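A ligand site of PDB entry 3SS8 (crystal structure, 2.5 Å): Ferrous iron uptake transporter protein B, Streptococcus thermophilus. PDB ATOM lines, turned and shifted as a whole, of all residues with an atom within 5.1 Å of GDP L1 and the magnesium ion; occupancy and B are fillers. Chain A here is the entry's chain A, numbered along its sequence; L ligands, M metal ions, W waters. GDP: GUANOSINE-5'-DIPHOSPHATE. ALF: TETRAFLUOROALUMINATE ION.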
ATOM      1  N   ASN A  11       5.923  -6.305 -17.199  1.00  0.00           N
ATOM      2  CA  ASN A  11       7.208  -6.993 -17.314  1.00  0.00           C
ATOM      3  C   ASN A  11       8.341  -6.061 -16.947  1.00  0.00           C
ATOM      4  O   ASN A  11       8.167  -4.839 -17.016  1.00  0.00           O
ATOM      5  CB  ASN A  11       7.435  -7.499 -18.742  1.00  0.00           C
ATOM      6  CG  ASN A  11       6.580  -8.720 -19.116  1.00  0.00           C
ATOM      7  OD1 ASN A  11       6.665  -9.184 -20.242  1.00  0.00           O
ATOM      8  ND2 ASN A  11       5.774  -9.230 -18.179  1.00  0.00           N
ATOM      9  N   PRO A  12       9.507  -6.620 -16.530  1.00  0.00           N
ATOM     10  CA  PRO A  12      10.644  -5.725 -16.345  1.00  0.00           C
ATOM     11  C   PRO A  12      11.032  -5.027 -17.648  1.00  0.00           C
ATOM     12  O   PRO A  12      10.877  -5.610 -18.719  1.00  0.00           O
ATOM     13  CB  PRO A  12      11.766  -6.673 -15.893  1.00  0.00           C
ATOM     14  CG  PRO A  12      11.061  -7.853 -15.327  1.00  0.00           C
ATOM     15  CD  PRO A  12       9.836  -8.010 -16.164  1.00  0.00           C
ATOM     16  N   ASN A  13      11.506  -3.785 -17.535  1.00  0.00           N
ATOM     17  CA  ASN A  13      12.048  -3.007 -18.682  1.00  0.00           C
ATOM     18  C   ASN A  13      10.963  -2.524 -19.662  1.00  0.00           C
ATOM     19  O   ASN A  13      11.264  -2.169 -20.804  1.00  0.00           O
ATOM     20  CB  ASN A  13      13.178  -3.814 -19.396  1.00  0.00           C
ATOM     21  CG  ASN A  13      14.434  -2.979 -19.657  1.00  0.00           C
ATOM     22  OD1 ASN A  13      14.670  -1.946 -19.029  1.00  0.00           O
ATOM     23  ND2 ASN A  13      15.264  -3.445 -20.587  1.00  0.00           N
ATOM     24  N   SER A  14       9.713  -2.501 -19.200  1.00  0.00           N
ATOM     25  CA  SER A  14       8.555  -2.074 -20.007  1.00  0.00           C
ATOM     26  C   SER A  14       8.354  -0.559 -20.016  1.00  0.00           C
ATOM     27  O   SER A  14       7.647  -0.030 -20.888  1.00  0.00           O
ATOM     28  CB  SER A  14       7.281  -2.789 -19.535  1.00  0.00           C
ATOM     29  OG  SER A  14       7.094  -2.685 -18.130  1.00  0.00           O
ATOM     30  N   GLY A  15       8.971   0.122 -19.050  1.00  0.00           N
ATOM     31  CA  GLY A  15       8.931   1.586 -18.968  1.00  0.00           C
ATOM     32  C   GLY A  15       8.036   2.128 -17.871  1.00  0.00           C
ATOM     33  O   GLY A  15       7.541   3.251 -17.985  1.00  0.00           O
ATOM     34  N   LYS A  16       7.830   1.344 -16.815  1.00  0.00           N
ATOM     35  CA  LYS A  16       6.944   1.693 -15.699  1.00  0.00           C
ATOM     36  C   LYS A  16       7.401   2.933 -14.940  1.00  0.00           C
ATOM     37  O   LYS A  16       6.599   3.858 -14.731  1.00  0.00           O
ATOM     38  CB  LYS A  16       6.795   0.527 -14.710  1.00  0.00           C
ATOM     39  CG  LYS A  16       6.034  -0.681 -15.232  1.00  0.00           C
ATOM     40  CD  LYS A  16       5.996  -1.845 -14.220  1.00  0.00           C
ATOM     41  CE  LYS A  16       7.394  -2.364 -13.901  1.00  0.00           C
ATOM     42  NZ  LYS A  16       8.146  -2.865 -15.081  1.00  0.00           N
ATOM     43  N   THR A  17       8.676   2.960 -14.539  1.00  0.00           N
ATOM     44  CA  THR A  17       9.232   4.105 -13.809  1.00  0.00           C
ATOM     45  C   THR A  17       9.297   5.364 -14.693  1.00  0.00           C
ATOM     46  O   THR A  17       9.112   6.474 -14.178  1.00  0.00           O
ATOM     47  CB  THR A  17      10.613   3.797 -13.192  1.00  0.00           C
ATOM     48  OG1 THR A  17      10.576   2.499 -12.582  1.00  0.00           O
ATOM     49  CG2 THR A  17      10.984   4.822 -12.125  1.00  0.00           C
ATOM     50  N   SER A  18       9.552   5.179 -15.991  1.00  0.00           N
ATOM     51  CA  SER A  18       9.550   6.283 -16.963  1.00  0.00           C
ATOM     52  C   SER A  18       8.202   6.991 -16.976  1.00  0.00           C
ATOM     53  O   SER A  18       8.128   8.221 -16.966  1.00  0.00           O
ATOM     54  CB  SER A  18       9.904   5.783 -18.362  1.00  0.00           C
ATOM     55  OG  SER A  18      11.215   5.252 -18.431  1.00  0.00           O
ATOM     56  N   ARG A  29      14.629   6.078 -10.153  1.00  0.00           N
ATOM     57  CA  ARG A  29      15.638   5.432 -11.004  1.00  0.00           C
ATOM     58  C   ARG A  29      15.055   4.696 -12.217  1.00  0.00           C
ATOM     59  O   ARG A  29      14.215   3.794 -12.084  1.00  0.00           O
ATOM     60  CB  ARG A  29      16.544   4.532 -10.162  1.00  0.00           C
ATOM     61  CG  ARG A  29      17.429   5.284  -9.161  1.00  0.00           C
ATOM     62  CD  ARG A  29      18.554   4.427  -8.581  1.00  0.00           C
ATOM     63  NE  ARG A  29      19.513   5.260  -7.838  1.00  0.00           N
ATOM     64  CZ  ARG A  29      20.694   4.871  -7.372  1.00  0.00           C
ATOM     65  NH1 ARG A  29      21.138   3.627  -7.536  1.00  0.00           N
ATOM     66  NH2 ARG A  29      21.457   5.741  -6.719  1.00  0.00           N
ATOM     67  N   VAL A  30      15.532   5.116 -13.393  1.00  0.00           N
ATOM     68  CA  VAL A  30      15.191   4.558 -14.704  1.00  0.00           C
ATOM     69  C   VAL A  30      16.484   4.095 -15.371  1.00  0.00           C
ATOM     70  O   VAL A  30      17.415   4.880 -15.532  1.00  0.00           O
ATOM     71  CB  VAL A  30      14.473   5.594 -15.624  1.00  0.00           C
ATOM     72  CG1 VAL A  30      14.301   5.083 -17.054  1.00  0.00           C
ATOM     73  CG2 VAL A  30      13.116   5.994 -15.063  1.00  0.00           C
ATOM     74  N   GLY A  31      16.543   2.826 -15.756  1.00  0.00           N
ATOM     75  CA  GLY A  31      17.700   2.248 -16.428  1.00  0.00           C
ATOM     76  C   GLY A  31      17.267   1.335 -17.553  1.00  0.00           C
ATOM     77  O   GLY A  31      16.163   0.784 -17.506  1.00  0.00           O
ATOM     78  N   ASN A  32      18.136   1.164 -18.558  1.00  0.00           N
ATOM     79  CA  ASN A  32      17.817   0.374 -19.746  1.00  0.00           C
ATOM     80  C   ASN A  32      18.152  -1.117 -19.640  1.00  0.00           C
ATOM     81  O   ASN A  32      18.537  -1.743 -20.631  1.00  0.00           O
ATOM     82  CB  ASN A  32      18.462   1.005 -20.998  1.00  0.00           C
ATOM     83  CG  ASN A  32      19.996   1.070 -20.909  1.00  0.00           C
ATOM     84  OD1 ASN A  32      20.583   1.048 -19.827  1.00  0.00           O
ATOM     85  ND2 ASN A  32      20.627   1.174 -22.066  1.00  0.00           N
ATOM     86  N   VAL A  36      15.951  -2.506 -12.209  1.00  0.00           N
ATOM     87  CA  VAL A  36      16.349  -1.278 -11.503  1.00  0.00           C
ATOM     88  C   VAL A  36      15.425  -1.063 -10.303  1.00  0.00           C
ATOM     89  O   VAL A  36      15.910  -1.061  -9.170  1.00  0.00           O
ATOM     90  CB  VAL A  36      16.415  -0.036 -12.460  1.00  0.00           C
ATOM     91  CG1 VAL A  36      16.694   1.247 -11.710  1.00  0.00           C
ATOM     92  CG2 VAL A  36      17.481  -0.244 -13.538  1.00  0.00           C
ATOM     93  N   THR A  37      14.121  -0.906 -10.536  1.00  0.00           N
ATOM     94  CA  THR A  37      13.121  -0.751  -9.459  1.00  0.00           C
ATOM     95  C   THR A  37      13.024  -2.081  -8.726  1.00  0.00           C
ATOM     96  O   THR A  37      12.728  -3.108  -9.335  1.00  0.00           O
ATOM     97  CB  THR A  37      11.710  -0.349  -9.980  1.00  0.00           C
ATOM     98  OG1 THR A  37      11.808   0.693 -10.956  1.00  0.00           O
ATOM     99  CG2 THR A  37      10.765   0.059  -8.833  1.00  0.00           C
ATOM    100  N   ASP A  55       4.534   2.663  -8.209  1.00  0.00           N
ATOM    101  CA  ASP A  55       5.543   2.059  -9.071  1.00  0.00           C
ATOM    102  C   ASP A  55       6.028   0.802  -8.375  1.00  0.00           C
ATOM    103  O   ASP A  55       6.383   0.828  -7.200  1.00  0.00           O
ATOM    104  CB  ASP A  55       6.708   3.008  -9.380  1.00  0.00           C
ATOM    105  CG  ASP A  55       7.645   2.462 -10.469  1.00  0.00           C
ATOM    106  OD1 ASP A  55       7.200   1.675 -11.337  1.00  0.00           O
ATOM    107  OD2 ASP A  55       8.846   2.829 -10.453  1.00  0.00           O
ATOM    108  N   LEU A  56       6.018  -0.303  -9.110  1.00  0.00           N
ATOM    109  CA  LEU A  56       6.399  -1.600  -8.560  1.00  0.00           C
ATOM    110  C   LEU A  56       7.473  -2.236  -9.438  1.00  0.00           C
ATOM    111  O   LEU A  56       7.606  -1.862 -10.615  1.00  0.00           O
ATOM    112  CB  LEU A  56       5.151  -2.486  -8.420  1.00  0.00           C
ATOM    113  CG  LEU A  56       4.206  -2.098  -7.260  1.00  0.00           C
ATOM    114  CD1 LEU A  56       2.761  -2.410  -7.581  1.00  0.00           C
ATOM    115  CD2 LEU A  56       4.605  -2.718  -5.920  1.00  0.00           C
ATOM    116  N   ASN A 115       2.937   0.838 -24.150  1.00  0.00           N
ATOM    117  CA  ASN A 115       4.150   1.643 -24.136  1.00  0.00           C
ATOM    118  C   ASN A 115       5.125   1.310 -25.261  1.00  0.00           C
ATOM    119  O   ASN A 115       5.008   0.249 -25.897  1.00  0.00           O
ATOM    120  CB  ASN A 115       4.842   1.499 -22.771  1.00  0.00           C
ATOM    121  CG  ASN A 115       5.714   2.697 -22.427  1.00  0.00           C
ATOM    122  OD1 ASN A 115       5.330   3.860 -22.623  1.00  0.00           O
ATOM    123  ND2 ASN A 115       6.899   2.426 -21.900  1.00  0.00           N
ATOM    124  N   MET A 116       6.074   2.221 -25.483  1.00  0.00           N
ATOM    125  CA  MET A 116       7.120   2.127 -26.501  1.00  0.00           C
ATOM    126  C   MET A 116       6.559   2.042 -27.924  1.00  0.00           C
ATOM    127  O   MET A 116       7.133   1.389 -28.796  1.00  0.00           O
ATOM    128  CB  MET A 116       8.096   0.969 -26.211  1.00  0.00           C
ATOM    129  CG  MET A 116       8.962   1.271 -25.021  1.00  0.00           C
ATOM    130  SD  MET A 116       9.834  -0.159 -24.441  1.00  0.00           S
ATOM    131  CE  MET A 116      10.481   0.461 -22.894  1.00  0.00           C
ATOM    132  N   ILE A 117       5.422   2.722 -28.132  1.00  0.00           N
ATOM    133  CA  ILE A 117       4.754   2.800 -29.436  1.00  0.00           C
ATOM    134  C   ILE A 117       5.661   3.489 -30.483  1.00  0.00           C
ATOM    135  O   ILE A 117       5.548   3.195 -31.681  1.00  0.00           O
ATOM    136  CB  ILE A 117       3.322   3.453 -29.313  1.00  0.00           C
ATOM    137  CG1 ILE A 117       2.416   3.058 -30.487  1.00  0.00           C
ATOM    138  CG2 ILE A 117       3.376   4.970 -29.081  1.00  0.00           C
ATOM    139  CD1 ILE A 117       1.800   1.660 -30.366  1.00  0.00           C
ATOM    140  N   ASP A 118       6.552   4.373 -30.018  1.00  0.00           N
ATOM    141  CA  ASP A 118       7.530   5.091 -30.844  1.00  0.00           C
ATOM    142  C   ASP A 118       8.552   4.171 -31.537  1.00  0.00           C
ATOM    143  O   ASP A 118       8.859   4.377 -32.713  1.00  0.00           O
ATOM    144  CB  ASP A 118       8.256   6.187 -30.029  1.00  0.00           C
ATOM    145  CG  ASP A 118       8.982   5.637 -28.804  1.00  0.00           C
ATOM    146  OD1 ASP A 118       8.323   5.118 -27.881  1.00  0.00           O
ATOM    147  OD2 ASP A 118      10.223   5.734 -28.751  1.00  0.00           O
ATOM    148  N   VAL A 119       9.044   3.170 -30.791  1.00  0.00           N
ATOM    149  CA  VAL A 119       9.992   2.154 -31.284  1.00  0.00           C
ATOM    150  C   VAL A 119       9.295   1.300 -32.344  1.00  0.00           C
ATOM    151  O   VAL A 119       9.880   0.989 -33.381  1.00  0.00           O
ATOM    152  CB  VAL A 119      10.540   1.230 -30.149  1.00  0.00           C
ATOM    153  CG1 VAL A 119      11.667   0.322 -30.646  1.00  0.00           C
ATOM    154  CG2 VAL A 119      11.035   2.035 -28.949  1.00  0.00           C
ATOM    155  N   THR A 143       1.000   4.477 -25.821  1.00  0.00           N
ATOM    156  CA  THR A 143       1.793   5.478 -25.102  1.00  0.00           C
ATOM    157  C   THR A 143       3.281   5.436 -25.462  1.00  0.00           C
ATOM    158  O   THR A 143       3.803   4.426 -25.943  1.00  0.00           O
ATOM    159  CB  THR A 143       1.667   5.337 -23.553  1.00  0.00           C
ATOM    160  OG1 THR A 143       2.127   4.037 -23.138  1.00  0.00           O
ATOM    161  CG2 THR A 143       0.241   5.533 -23.057  1.00  0.00           C
ATOM    162  N   SER A 144       3.946   6.565 -25.226  1.00  0.00           N
ATOM    163  CA  SER A 144       5.390   6.687 -25.335  1.00  0.00           C
ATOM    164  C   SER A 144       5.860   7.561 -24.179  1.00  0.00           C
ATOM    165  O   SER A 144       5.408   8.705 -24.044  1.00  0.00           O
ATOM    166  CB  SER A 144       5.808   7.261 -26.685  1.00  0.00           C
ATOM    167  OG  SER A 144       7.216   7.437 -26.768  1.00  0.00           O
ATOM    168  N   ALA A 145       6.745   7.018 -23.348  1.00  0.00           N
ATOM    169  CA  ALA A 145       7.341   7.785 -22.254  1.00  0.00           C
ATOM    170  C   ALA A 145       8.427   8.723 -22.794  1.00  0.00           C
ATOM    171  O   ALA A 145       8.637   9.812 -22.250  1.00  0.00           O
ATOM    172  CB  ALA A 145       7.919   6.853 -21.221  1.00  0.00           C
ATOM    173  N   LEU A 146       9.084   8.284 -23.870  1.00  0.00           N
ATOM    174  CA  LEU A 146      10.130   9.042 -24.552  1.00  0.00           C
ATOM    175  C   LEU A 146       9.541  10.292 -25.206  1.00  0.00           C
ATOM    176  O   LEU A 146       9.979  11.403 -24.932  1.00  0.00           O
ATOM    177  CB  LEU A 146      10.835   8.151 -25.591  1.00  0.00           C
ATOM    178  CG  LEU A 146      12.241   8.519 -26.083  1.00  0.00           C
ATOM    179  CD1 LEU A 146      13.305   8.138 -25.065  1.00  0.00           C
ATOM    180  CD2 LEU A 146      12.538   7.831 -27.397  1.00  0.00           C
HETATM  181  PB  GDP L   1      10.720  -0.303 -15.916  1.00  0.00           P
HETATM  182  O1B GDP L   1       9.425  -0.942 -16.299  1.00  0.00           O
HETATM  183  O2B GDP L   1      11.782  -1.368 -15.336  1.00  0.00           O
HETATM  184  O3B GDP L   1      10.547   0.804 -14.747  1.00  0.00           O
HETATM  185  O3A GDP L   1      11.431   0.415 -17.164  1.00  0.00           O
HETATM  186  PA  GDP L   1      12.139   1.885 -17.044  1.00  0.00           P
HETATM  187  O1A GDP L   1      11.227   2.946 -16.543  1.00  0.00           O
HETATM  188  O2A GDP L   1      13.435   1.665 -16.087  1.00  0.00           O
HETATM  189  O5' GDP L   1      12.694   2.198 -18.482  1.00  0.00           O
HETATM  190  C5' GDP L   1      13.231   1.136 -19.311  1.00  0.00           C
HETATM  191  C4' GDP L   1      14.031   1.692 -20.487  1.00  0.00           C
HETATM  192  O4' GDP L   1      13.006   2.012 -21.420  1.00  0.00           O
HETATM  193  C3' GDP L   1      14.773   3.006 -20.177  1.00  0.00           C
HETATM  194  O3' GDP L   1      16.004   2.988 -20.903  1.00  0.00           O
HETATM  195  C2' GDP L   1      13.844   4.106 -20.696  1.00  0.00           C
HETATM  196  O2' GDP L   1      14.607   5.191 -21.189  1.00  0.00           O
HETATM  197  C1' GDP L   1      13.137   3.398 -21.838  1.00  0.00           C
HETATM  198  N9  GDP L   1      11.723   3.721 -22.139  1.00  0.00           N
HETATM  199  C8  GDP L   1      10.686   3.761 -21.318  1.00  0.00           C
HETATM  200  N7  GDP L   1       9.590   4.070 -22.014  1.00  0.00           N
HETATM  201  C5  GDP L   1       9.934   4.226 -23.286  1.00  0.00           C
HETATM  202  C6  GDP L   1       9.223   4.546 -24.453  1.00  0.00           C
HETATM  203  O6  GDP L   1       8.011   4.756 -24.431  1.00  0.00           O
HETATM  204  N1  GDP L   1       9.914   4.610 -25.672  1.00  0.00           N
HETATM  205  C2  GDP L   1      11.292   4.361 -25.685  1.00  0.00           C
HETATM  206  N2  GDP L   1      11.983   4.430 -26.812  1.00  0.00           N
HETATM  207  N3  GDP L   1      11.945   4.062 -24.547  1.00  0.00           N
HETATM  208  C4  GDP L   1      11.300   3.987 -23.371  1.00  0.00           C
HETATM  209 AL   ALF L   2      12.221  -2.456 -13.866  1.00  0.00          AL
HETATM  210  F1  ALF L   2      10.594  -3.136 -14.121  1.00  0.00           F
HETATM  211  F2  ALF L   2      13.848  -1.775 -13.593  1.00  0.00           F
HETATM  212  F3  ALF L   2      12.929  -3.789 -14.844  1.00  0.00           F
HETATM  213  F4  ALF L   2      11.538  -1.142 -12.890  1.00  0.00           F
HETATM  214 MG    MG M   1      10.911   0.528 -12.917  1.00  0.00          MG
HETATM  215  O   HOH W   1       9.153  -0.011 -12.165  1.00  0.00           O
HETATM  216  O   HOH W   2      12.879   1.442 -13.454  1.00  0.00           O
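Val 30 touches GDP L1.
CB of Asn 32 touches O3' of GDP L1, 3.2 Å away.
Val 119 touches GDP L1.
Ser 144 touches GDP L1.
Leu 146 touches GDP L1.
Of the 25 residues printed, 17 come within 4 Å of GDP L1.
The backbone carbonyl oxygen of Gly 31 sits close to the side-chain amide oxygen of Asn 13.
The side-chain hydroxyl (OG1) of Thr 143 sits at hydrogen-bond distance from the side-chain amide oxygen (OD1) of Asn 115, 3.2 Å away.
NZ of Lys 16 lies within hydrogen-bond range of O of Asn 11, 2.8 Å away.
The backbone carbonyl oxygen (O) of Thr 143 lies within hydrogen-bond range of the backbone NH (N) of Met 116.
The side-chain hydroxyl (OG) of Ser 14 sits at hydrogen-bond distance from the backbone carbonyl oxygen (O) of Asn 11, 2.7 Å away.
OD2 of Asp 55 sits close to OG1 of Thr 17, 2.8 Å away.
The side-chain carboxylate of Asp 118 is in hydrogen-bond range of the side-chain hydroxyl of Ser 144 (2.8 Å).
The side-chain hydroxyl (OG) of Ser 14 lies within hydrogen-bond range of the side-chain amino group (NZ) of Lys 16, at 3.2 Å.
Merely in contact with the magnesium ion: Asp 55 (3.95 Å).
The nearest printed residue that does not touch the magnesium ion is Lys 16 (4.5 Å).
An oxygen (O2B) of GDP L1 binds an aluminium atom (AL) of ALF L2 (1.9 Å).
The magnesium ion is bound by F4 of ALF L2 (1.8 Å), O3B of GDP L1 (1.9 Å), water W1 (2.0 Å), OG1 of Thr 17 (2.0 Å), OG1 of Thr 37 (2.2 Å) and water W2 (2.2 Å).
The magnesium ion has six donor atoms within binding distance.
O1A of GDP L1 is in hydrogen-bond range of OG of Ser 18 (3.0 Å).
The side-chain amino group (NZ) of Lys 16 lies within salt-bridge range of an oxygen (O1B) of GDP L1, 2.6 Å away.
The backbone NH (N) of Gly 15 is in hydrogen-bond range of an oxygen (O1B) of GDP L1 (3.0 Å).
The backbone NH (N) of Asn 13 lies within hydrogen-bond range of a fluorine (F3) of ALF L2 (3.0 Å).
A nitrogen (N7) of GDP L1 lies within hydrogen-bond range of the side-chain amide nitrogen of Asn 115 (3.2 Å).
The backbone NH (N) of Thr 37 sits at hydrogen-bond distance from a fluorine (F2) of ALF L2 (3.2 Å).
An oxygen (O1B) of GDP L1 is in hydrogen-bond range of the backbone NH (N) of Ser 14, 3.3 Å away.
F2 of ALF L2 sits at hydrogen-bond distance from N of Val 36 (2.6 Å).
The side-chain amino group (NZ) of Lys 16 is in hydrogen-bond range of a fluorine (F1) of ALF L2, 2.6 Å away.
The backbone NH (N) of Ser 18 is in hydrogen-bond range of an oxygen (O1A) of GDP L1 (2.8 Å).
N of Thr 17 sits at hydrogen-bond distance from O1A of GDP L1 (3.2 Å).
The backbone NH (N) of Lys 16 sits at hydrogen-bond distance from an oxygen (O1B) of GDP L1, at 2.8 Å.
O6 of GDP L1 sits at hydrogen-bond distance from N of Ala 145, 2.8 Å away.
N of Asn 13 sits close to O2B of GDP L1 (3.3 Å).
A nitrogen (N1) of GDP L1 lies within hydrogen-bond range of the side-chain carboxylate of Asp 118, 2.8 Å away.
N of Gly 31 lies within hydrogen-bond range of O2A of GDP L1 (3.3 Å).
The side-chain hydroxyl of Ser 14 lies within hydrogen-bond range of an oxygen (O1B) of GDP L1, at 3.4 Å.
An oxygen (O6) of GDP L1 sits at hydrogen-bond distance from the backbone NH of Met 116.
Water W2 lies within hydrogen-bond range of an oxygen (O2A) of GDP L1 and the backbone carbonyl oxygen (O) of Arg 29.
Water W1 lies within hydrogen-bond range of OD1 of Asp 55 (2.7 Å) and O of Leu 56 (2.9 Å).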
